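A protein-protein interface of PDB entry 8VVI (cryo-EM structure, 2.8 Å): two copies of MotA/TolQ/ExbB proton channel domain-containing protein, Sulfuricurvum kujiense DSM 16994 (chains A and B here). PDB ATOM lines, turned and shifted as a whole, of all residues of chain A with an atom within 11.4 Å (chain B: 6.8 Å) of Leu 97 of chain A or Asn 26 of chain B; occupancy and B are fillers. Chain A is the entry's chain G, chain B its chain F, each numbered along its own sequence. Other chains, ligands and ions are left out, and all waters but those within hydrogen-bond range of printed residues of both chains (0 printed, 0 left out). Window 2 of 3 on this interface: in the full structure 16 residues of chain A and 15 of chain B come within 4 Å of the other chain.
The backbone carbonyl oxygen (O) of Leu 97 of chain A is in hydrogen-bond range of the side-chain amide nitrogen (ND2) of Asn 26 of chain B, 3.3 Å away.
Of the 9 printed residues of chain B, 4 touch a printed residue of chain A.
Hydrophobic or aromatic side chains of chain B that line the printed part of chain A: Ile 29 and Leu 32.
Among the printed residues, no Asp or Glu carboxylate lies within 4 Å of a Lys or Arg side-chain nitrogen of the other chain.
2 positions are printed for both chains.
Of the 6 pairs that touch across the chains among the printed residues, none has its exchanged pair printed and touching as well.
Lys 90 of chain A touches none of the printed residues of chain B.
Leu 92 of chain A touches none of the printed residues of chain B.
Of the printed residues of chain B, Ile 94 of chain A touches Ile 29.
Of chain B, only Asn 26, Ser 28, Ile 29 and Leu 32 come within 4 Å of Leu 97 of chain A.
Of the printed residues of chain B, Thr 98 of chain A touches Ile 29 (3.7 Å).
No residue of chain A comes within 4 Å of Asn 23 of chain B.
No residue of chain A comes within 4 Å of Arg 25 of chain B.
Of chain A, only Leu 97 (3.3 Å) comes within 4 Å of Asn 26 of chain B.
No residue of chain A comes within 4 Å of Lys 27 of chain B.
Ser 28 of chain B touches just one residue of chain A: Leu 97.
Of the printed residues of chain A, Ile 29 of chain B touches Ile 94 (3.7 Å), Leu 97 (3.8 Å) and Thr 98 (3.7 Å).
Printed residues of chain A within 4 Å of Leu 32 of chain B: Leu 97 (3.9 Å).
The nearest residue of chain B that does not touch Leu 97 of chain A is Gln 30 of chain B (6.3 Å).
The nearest residue of chain A that does not touch Asn 26 of chain B is Thr 98 of chain A (4.7 Å).
The nearest printed residue of chain A that does not touch Leu 32 of chain B is Ile 94 of chain A (5.1 Å).
The backbone carbonyl oxygen (O) of Phe 95 of chain A lies within hydrogen-bond range of the side-chain hydroxyl (OG1) of Thr 98 of chain A, at 3.1 Å.
OG1 of Thr 98 of chain A lies within hydrogen-bond range of NH1 of Arg 99 of chain A (2.8 Å).
Ile 94 of chain A touches Ile 29 of chain B.
OG of Ser 28 of chain B touches CD2 of Leu 97 of chain A (3.5 Å).
Leu 97 of chain A touches Ile 29 of chain B (CB to CG1, 3.8 Å).
CD1 of Leu 97 of chain A touches CD1 of Leu 32 of chain B (3.9 Å).
Thr 98 of chain A touches Ile 29 of chain B.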
ATOM      1  N   ARG A  24      21.383   9.747  -7.511  1.00  0.00           N
ATOM      2  CA  ARG A  24      20.723  10.909  -8.102  1.00  0.00           C
ATOM      3  C   ARG A  24      21.142  12.219  -7.431  1.00  0.00           C
ATOM      4  O   ARG A  24      20.706  13.301  -7.835  1.00  0.00           O
ATOM      5  CB  ARG A  24      19.202  10.715  -8.044  1.00  0.00           C
ATOM      6  CG  ARG A  24      18.360  11.735  -8.803  1.00  0.00           C
ATOM      7  CD  ARG A  24      18.634  11.698 -10.298  1.00  0.00           C
ATOM      8  NE  ARG A  24      19.560  12.745 -10.709  1.00  0.00           N
ATOM      9  CZ  ARG A  24      20.066  12.864 -11.929  1.00  0.00           C
ATOM     10  NH1 ARG A  24      19.763  12.006 -12.889  1.00  0.00           N
ATOM     11  NH2 ARG A  24      20.895  13.869 -12.194  1.00  0.00           N
ATOM     12  N   LYS A  27      26.278  13.811  -7.611  1.00  0.00           N
ATOM     13  CA  LYS A  27      26.777  14.786  -8.578  1.00  0.00           C
ATOM     14  C   LYS A  27      28.131  14.395  -9.155  1.00  0.00           C
ATOM     15  O   LYS A  27      28.623  15.079 -10.061  1.00  0.00           O
ATOM     16  CB  LYS A  27      26.871  16.206  -7.997  1.00  0.00           C
ATOM     17  CG  LYS A  27      25.590  16.696  -7.340  1.00  0.00           C
ATOM     18  CD  LYS A  27      24.419  16.645  -8.307  1.00  0.00           C
ATOM     19  CE  LYS A  27      23.114  17.001  -7.613  1.00  0.00           C
ATOM     20  NZ  LYS A  27      21.930  16.645  -8.442  1.00  0.00           N
ATOM     21  N   ILE A  88      18.250  10.129 -20.496  1.00  0.00           N
ATOM     22  CA  ILE A  88      17.410  10.419 -19.337  1.00  0.00           C
ATOM     23  C   ILE A  88      18.231  11.070 -18.233  1.00  0.00           C
ATOM     24  O   ILE A  88      17.789  12.035 -17.597  1.00  0.00           O
ATOM     25  CB  ILE A  88      16.716   9.134 -18.849  1.00  0.00           C
ATOM     26  CG1 ILE A  88      15.785   8.587 -19.931  1.00  0.00           C
ATOM     27  CG2 ILE A  88      15.945   9.395 -17.565  1.00  0.00           C
ATOM     28  CD1 ILE A  88      15.024   7.352 -19.511  1.00  0.00           C
ATOM     29  N   ILE A  89      19.436  10.555 -17.986  1.00  0.00           N
ATOM     30  CA  ILE A  89      20.313  11.159 -16.987  1.00  0.00           C
ATOM     31  C   ILE A  89      20.684  12.580 -17.396  1.00  0.00           C
ATOM     32  O   ILE A  89      20.678  13.502 -16.572  1.00  0.00           O
ATOM     33  CB  ILE A  89      21.561  10.285 -16.772  1.00  0.00           C
ATOM     34  CG1 ILE A  89      21.164   8.911 -16.228  1.00  0.00           C
ATOM     35  CG2 ILE A  89      22.538  10.966 -15.827  1.00  0.00           C
ATOM     36  CD1 ILE A  89      20.495   8.957 -14.873  1.00  0.00           C
ATOM     37  N   LYS A  90      21.013  12.778 -18.675  1.00  0.00           N
ATOM     38  CA  LYS A  90      21.332  14.116 -19.162  1.00  0.00           C
ATOM     39  C   LYS A  90      20.114  15.032 -19.114  1.00  0.00           C
ATOM     40  O   LYS A  90      20.232  16.211 -18.763  1.00  0.00           O
ATOM     41  CB  LYS A  90      21.891  14.038 -20.581  1.00  0.00           C
ATOM     42  CG  LYS A  90      23.238  13.344 -20.679  1.00  0.00           C
ATOM     43  CD  LYS A  90      24.003  13.796 -21.910  1.00  0.00           C
ATOM     44  CE  LYS A  90      23.895  12.776 -23.029  1.00  0.00           C
ATOM     45  NZ  LYS A  90      24.758  11.588 -22.781  1.00  0.00           N
ATOM     46  N   ILE A  91      18.939  14.511 -19.474  1.00  0.00           N
ATOM     47  CA  ILE A  91      17.719  15.311 -19.411  1.00  0.00           C
ATOM     48  C   ILE A  91      17.396  15.681 -17.969  1.00  0.00           C
ATOM     49  O   ILE A  91      16.989  16.813 -17.680  1.00  0.00           O
ATOM     50  CB  ILE A  91      16.554  14.561 -20.084  1.00  0.00           C
ATOM     51  CG1 ILE A  91      16.639  14.703 -21.605  1.00  0.00           C
ATOM     52  CG2 ILE A  91      15.214  15.066 -19.576  1.00  0.00           C
ATOM     53  CD1 ILE A  91      15.767  13.726 -22.358  1.00  0.00           C
ATOM     54  N   LEU A  92      17.575  14.738 -17.040  1.00  0.00           N
ATOM     55  CA  LEU A  92      17.352  15.039 -15.629  1.00  0.00           C
ATOM     56  C   LEU A  92      18.316  16.103 -15.125  1.00  0.00           C
ATOM     57  O   LEU A  92      17.972  16.873 -14.220  1.00  0.00           O
ATOM     58  CB  LEU A  92      17.481  13.766 -14.792  1.00  0.00           C
ATOM     59  CG  LEU A  92      16.278  12.821 -14.801  1.00  0.00           C
ATOM     60  CD1 LEU A  92      16.587  11.555 -14.019  1.00  0.00           C
ATOM     61  CD2 LEU A  92      15.046  13.514 -14.242  1.00  0.00           C
ATOM     62  N   ASP A  93      19.526  16.159 -15.686  1.00  0.00           N
ATOM     63  CA  ASP A  93      20.458  17.225 -15.330  1.00  0.00           C
ATOM     64  C   ASP A  93      19.931  18.585 -15.773  1.00  0.00           C
ATOM     65  O   ASP A  93      20.079  19.579 -15.054  1.00  0.00           O
ATOM     66  CB  ASP A  93      21.830  16.951 -15.943  1.00  0.00           C
ATOM     67  CG  ASP A  93      22.495  15.719 -15.359  1.00  0.00           C
ATOM     68  OD1 ASP A  93      21.914  15.107 -14.439  1.00  0.00           O
ATOM     69  OD2 ASP A  93      23.598  15.361 -15.823  1.00  0.00           O
ATOM     70  N   ILE A  94      19.322  18.648 -16.959  1.00  0.00           N
ATOM     71  CA  ILE A  94      18.712  19.891 -17.419  1.00  0.00           C
ATOM     72  C   ILE A  94      17.547  20.281 -16.517  1.00  0.00           C
ATOM     73  O   ILE A  94      17.389  21.454 -16.158  1.00  0.00           O
ATOM     74  CB  ILE A  94      18.268  19.763 -18.887  1.00  0.00           C
ATOM     75  CG1 ILE A  94      19.482  19.681 -19.809  1.00  0.00           C
ATOM     76  CG2 ILE A  94      17.372  20.925 -19.287  1.00  0.00           C
ATOM     77  CD1 ILE A  94      19.114  19.417 -21.241  1.00  0.00           C
ATOM     78  N   PHE A  95      16.715  19.307 -16.138  1.00  0.00           N
ATOM     79  CA  PHE A  95      15.568  19.600 -15.286  1.00  0.00           C
ATOM     80  C   PHE A  95      15.998  20.188 -13.948  1.00  0.00           C
ATOM     81  O   PHE A  95      15.266  20.992 -13.361  1.00  0.00           O
ATOM     82  CB  PHE A  95      14.740  18.334 -15.069  1.00  0.00           C
ATOM     83  CG  PHE A  95      13.360  18.598 -14.542  1.00  0.00           C
ATOM     84  CD1 PHE A  95      12.478  19.401 -15.246  1.00  0.00           C
ATOM     85  CD2 PHE A  95      12.943  18.044 -13.344  1.00  0.00           C
ATOM     86  CE1 PHE A  95      11.207  19.646 -14.766  1.00  0.00           C
ATOM     87  CE2 PHE A  95      11.673  18.284 -12.857  1.00  0.00           C
ATOM     88  CZ  PHE A  95      10.803  19.087 -13.570  1.00  0.00           C
ATOM     89  N   ASP A  96      17.175  19.804 -13.454  1.00  0.00           N
ATOM     90  CA  ASP A  96      17.710  20.392 -12.235  1.00  0.00           C
ATOM     91  C   ASP A  96      18.364  21.746 -12.470  1.00  0.00           C
ATOM     92  O   ASP A  96      18.608  22.474 -11.502  1.00  0.00           O
ATOM     93  CB  ASP A  96      18.720  19.438 -11.591  1.00  0.00           C
ATOM     94  CG  ASP A  96      18.120  18.083 -11.274  1.00  0.00           C
ATOM     95  OD1 ASP A  96      16.880  17.993 -11.161  1.00  0.00           O
ATOM     96  OD2 ASP A  96      18.889  17.109 -11.137  1.00  0.00           O
ATOM     97  N   LEU A  97      18.656  22.099 -13.721  1.00  0.00           N
ATOM     98  CA  LEU A  97      19.209  23.405 -14.048  1.00  0.00           C
ATOM     99  C   LEU A  97      18.144  24.486 -14.177  1.00  0.00           C
ATOM    100  O   LEU A  97      18.487  25.673 -14.174  1.00  0.00           O
ATOM    101  CB  LEU A  97      20.015  23.330 -15.349  1.00  0.00           C
ATOM    102  CG  LEU A  97      21.376  22.638 -15.269  1.00  0.00           C
ATOM    103  CD1 LEU A  97      21.997  22.514 -16.651  1.00  0.00           C
ATOM    104  CD2 LEU A  97      22.303  23.386 -14.326  1.00  0.00           C
ATOM    105  N   THR A  98      16.870  24.109 -14.292  1.00  0.00           N
ATOM    106  CA  THR A  98      15.792  25.086 -14.370  1.00  0.00           C
ATOM    107  C   THR A  98      15.403  25.645 -13.008  1.00  0.00           C
ATOM    108  O   THR A  98      14.622  26.600 -12.950  1.00  0.00           O
ATOM    109  CB  THR A  98      14.559  24.468 -15.036  1.00  0.00           C
ATOM    110  OG1 THR A  98      13.871  23.635 -14.096  1.00  0.00           O
ATOM    111  CG2 THR A  98      14.964  23.638 -16.242  1.00  0.00           C
ATOM    112  N   ARG A  99      15.922  25.079 -11.923  1.00  0.00           N
ATOM    113  CA  ARG A  99      15.624  25.568 -10.583  1.00  0.00           C
ATOM    114  C   ARG A  99      16.784  26.392 -10.038  1.00  0.00           C
ATOM    115  O   ARG A  99      17.915  25.914  -9.961  1.00  0.00           O
ATOM    116  CB  ARG A  99      15.316  24.403  -9.638  1.00  0.00           C
ATOM    117  CG  ARG A  99      13.931  23.798  -9.813  1.00  0.00           C
ATOM    118  CD  ARG A  99      13.906  22.747 -10.911  1.00  0.00           C
ATOM    119  NE  ARG A  99      12.648  22.011 -10.923  1.00  0.00           N
ATOM    120  CZ  ARG A  99      11.601  22.330 -11.672  1.00  0.00           C
ATOM    121  NH1 ARG A  99      11.632  23.363 -12.499  1.00  0.00           N
ATOM    122  NH2 ARG A  99      10.496  21.596 -11.590  1.00  0.00           N
ATOM    123  N   ASN B  23      14.543  28.460 -22.986  1.00  0.00           N
ATOM    124  CA  ASN B  23      15.445  28.537 -21.843  1.00  0.00           C
ATOM    125  C   ASN B  23      16.796  29.105 -22.264  1.00  0.00           C
ATOM    126  O   ASN B  23      17.835  28.726 -21.721  1.00  0.00           O
ATOM    127  CB  ASN B  23      15.617  27.165 -21.195  1.00  0.00           C
ATOM    128  CG  ASN B  23      14.365  26.692 -20.487  1.00  0.00           C
ATOM    129  OD1 ASN B  23      13.691  27.466 -19.809  1.00  0.00           O
ATOM    130  ND2 ASN B  23      14.044  25.414 -20.644  1.00  0.00           N
ATOM    131  N   ARG B  24      16.787  30.014 -23.242  1.00  0.00           N
ATOM    132  CA  ARG B  24      18.032  30.503 -23.826  1.00  0.00           C
ATOM    133  C   ARG B  24      18.814  31.384 -22.860  1.00  0.00           C
ATOM    134  O   ARG B  24      20.051  31.385 -22.890  1.00  0.00           O
ATOM    135  CB  ARG B  24      17.733  31.264 -25.120  1.00  0.00           C
ATOM    136  CG  ARG B  24      18.968  31.791 -25.823  1.00  0.00           C
ATOM    137  CD  ARG B  24      19.830  30.655 -26.337  1.00  0.00           C
ATOM    138  NE  ARG B  24      21.001  31.146 -27.054  1.00  0.00           N
ATOM    139  CZ  ARG B  24      22.001  30.379 -27.463  1.00  0.00           C
ATOM    140  NH1 ARG B  24      21.996  29.071 -27.263  1.00  0.00           N
ATOM    141  NH2 ARG B  24      23.036  30.939 -28.081  1.00  0.00           N
ATOM    142  N   ARG B  25      18.125  32.127 -21.996  1.00  0.00           N
ATOM    143  CA  ARG B  25      18.796  33.053 -21.093  1.00  0.00           C
ATOM    144  C   ARG B  25      19.495  32.358 -19.933  1.00  0.00           C
ATOM    145  O   ARG B  25      20.236  33.020 -19.197  1.00  0.00           O
ATOM    146  CB  ARG B  25      17.792  34.074 -20.552  1.00  0.00           C
ATOM    147  CG  ARG B  25      17.030  34.825 -21.633  1.00  0.00           C
ATOM    148  CD  ARG B  25      17.761  36.091 -22.054  1.00  0.00           C
ATOM    149  NE  ARG B  25      18.854  35.814 -22.979  1.00  0.00           N
ATOM    150  CZ  ARG B  25      18.703  35.615 -24.282  1.00  0.00           C
ATOM    151  NH1 ARG B  25      17.511  35.655 -24.854  1.00  0.00           N
ATOM    152  NH2 ARG B  25      19.775  35.369 -25.029  1.00  0.00           N
ATOM    153  N   ASN B  26      19.279  31.054 -19.746  1.00  0.00           N
ATOM    154  CA  ASN B  26      19.930  30.346 -18.649  1.00  0.00           C
ATOM    155  C   ASN B  26      21.441  30.292 -18.842  1.00  0.00           C
ATOM    156  O   ASN B  26      22.201  30.528 -17.895  1.00  0.00           O
ATOM    157  CB  ASN B  26      19.352  28.936 -18.525  1.00  0.00           C
ATOM    158  CG  ASN B  26      19.772  28.237 -17.243  1.00  0.00           C
ATOM    159  OD1 ASN B  26      20.530  28.781 -16.440  1.00  0.00           O
ATOM    160  ND2 ASN B  26      19.274  27.023 -17.043  1.00  0.00           N
ATOM    161  N   LYS B  27      21.893  29.973 -20.056  1.00  0.00           N
ATOM    162  CA  LYS B  27      23.293  29.827 -20.448  1.00  0.00           C
ATOM    163  C   LYS B  27      23.978  28.650 -19.765  1.00  0.00           C
ATOM    164  O   LYS B  27      25.154  28.390 -20.044  1.00  0.00           O
ATOM    165  CB  LYS B  27      24.114  31.101 -20.198  1.00  0.00           C
ATOM    166  CG  LYS B  27      23.679  32.288 -21.041  1.00  0.00           C
ATOM    167  CD  LYS B  27      24.466  33.539 -20.688  1.00  0.00           C
ATOM    168  CE  LYS B  27      24.014  34.725 -21.525  1.00  0.00           C
ATOM    169  NZ  LYS B  27      22.615  35.125 -21.210  1.00  0.00           N
ATOM    170  N   SER B  28      23.288  27.930 -18.884  1.00  0.00           N
ATOM    171  CA  SER B  28      23.768  26.669 -18.332  1.00  0.00           C
ATOM    172  C   SER B  28      23.085  25.469 -18.970  1.00  0.00           C
ATOM    173  O   SER B  28      23.732  24.448 -19.216  1.00  0.00           O
ATOM    174  CB  SER B  28      23.557  26.635 -16.816  1.00  0.00           C
ATOM    175  OG  SER B  28      24.291  25.577 -16.224  1.00  0.00           O
ATOM    176  N   ILE B  29      21.781  25.579 -19.237  1.00  0.00           N
ATOM    177  CA  ILE B  29      21.109  24.604 -20.091  1.00  0.00           C
ATOM    178  C   ILE B  29      21.725  24.626 -21.482  1.00  0.00           C
ATOM    179  O   ILE B  29      21.949  23.577 -22.099  1.00  0.00           O
ATOM    180  CB  ILE B  29      19.596  24.886 -20.128  1.00  0.00           C
ATOM    181  CG1 ILE B  29      18.909  24.266 -18.911  1.00  0.00           C
ATOM    182  CG2 ILE B  29      18.975  24.364 -21.415  1.00  0.00           C
ATOM    183  CD1 ILE B  29      17.451  24.636 -18.784  1.00  0.00           C
ATOM    184  N   GLN B  30      22.020  25.820 -21.990  1.00  0.00           N
ATOM    185  CA  GLN B  30      22.802  25.953 -23.206  1.00  0.00           C
ATOM    186  C   GLN B  30      24.214  25.424 -22.971  1.00  0.00           C
ATOM    187  O   GLN B  30      24.655  25.243 -21.832  1.00  0.00           O
ATOM    188  CB  GLN B  30      22.851  27.413 -23.655  1.00  0.00           C
ATOM    189  CG  GLN B  30      21.487  28.075 -23.785  1.00  0.00           C
ATOM    190  CD  GLN B  30      20.621  27.440 -24.854  1.00  0.00           C
ATOM    191  OE1 GLN B  30      21.107  27.059 -25.918  1.00  0.00           O
ATOM    192  NE2 GLN B  30      19.328  27.326 -24.577  1.00  0.00           N
ATOM    193  N   LEU B  32      24.976  22.632 -23.254  1.00  0.00           N
ATOM    194  CA  LEU B  32      24.650  21.222 -23.107  1.00  0.00           C
ATOM    195  C   LEU B  32      23.595  20.765 -24.099  1.00  0.00           C
ATOM    196  O   LEU B  32      23.503  19.565 -24.372  1.00  0.00           O
ATOM    197  CB  LEU B  32      24.151  20.928 -21.685  1.00  0.00           C
ATOM    198  CG  LEU B  32      25.126  21.113 -20.524  1.00  0.00           C
ATOM    199  CD1 LEU B  32      24.449  20.772 -19.207  1.00  0.00           C
ATOM    200  CD2 LEU B  32      26.361  20.256 -20.725  1.00  0.00           C
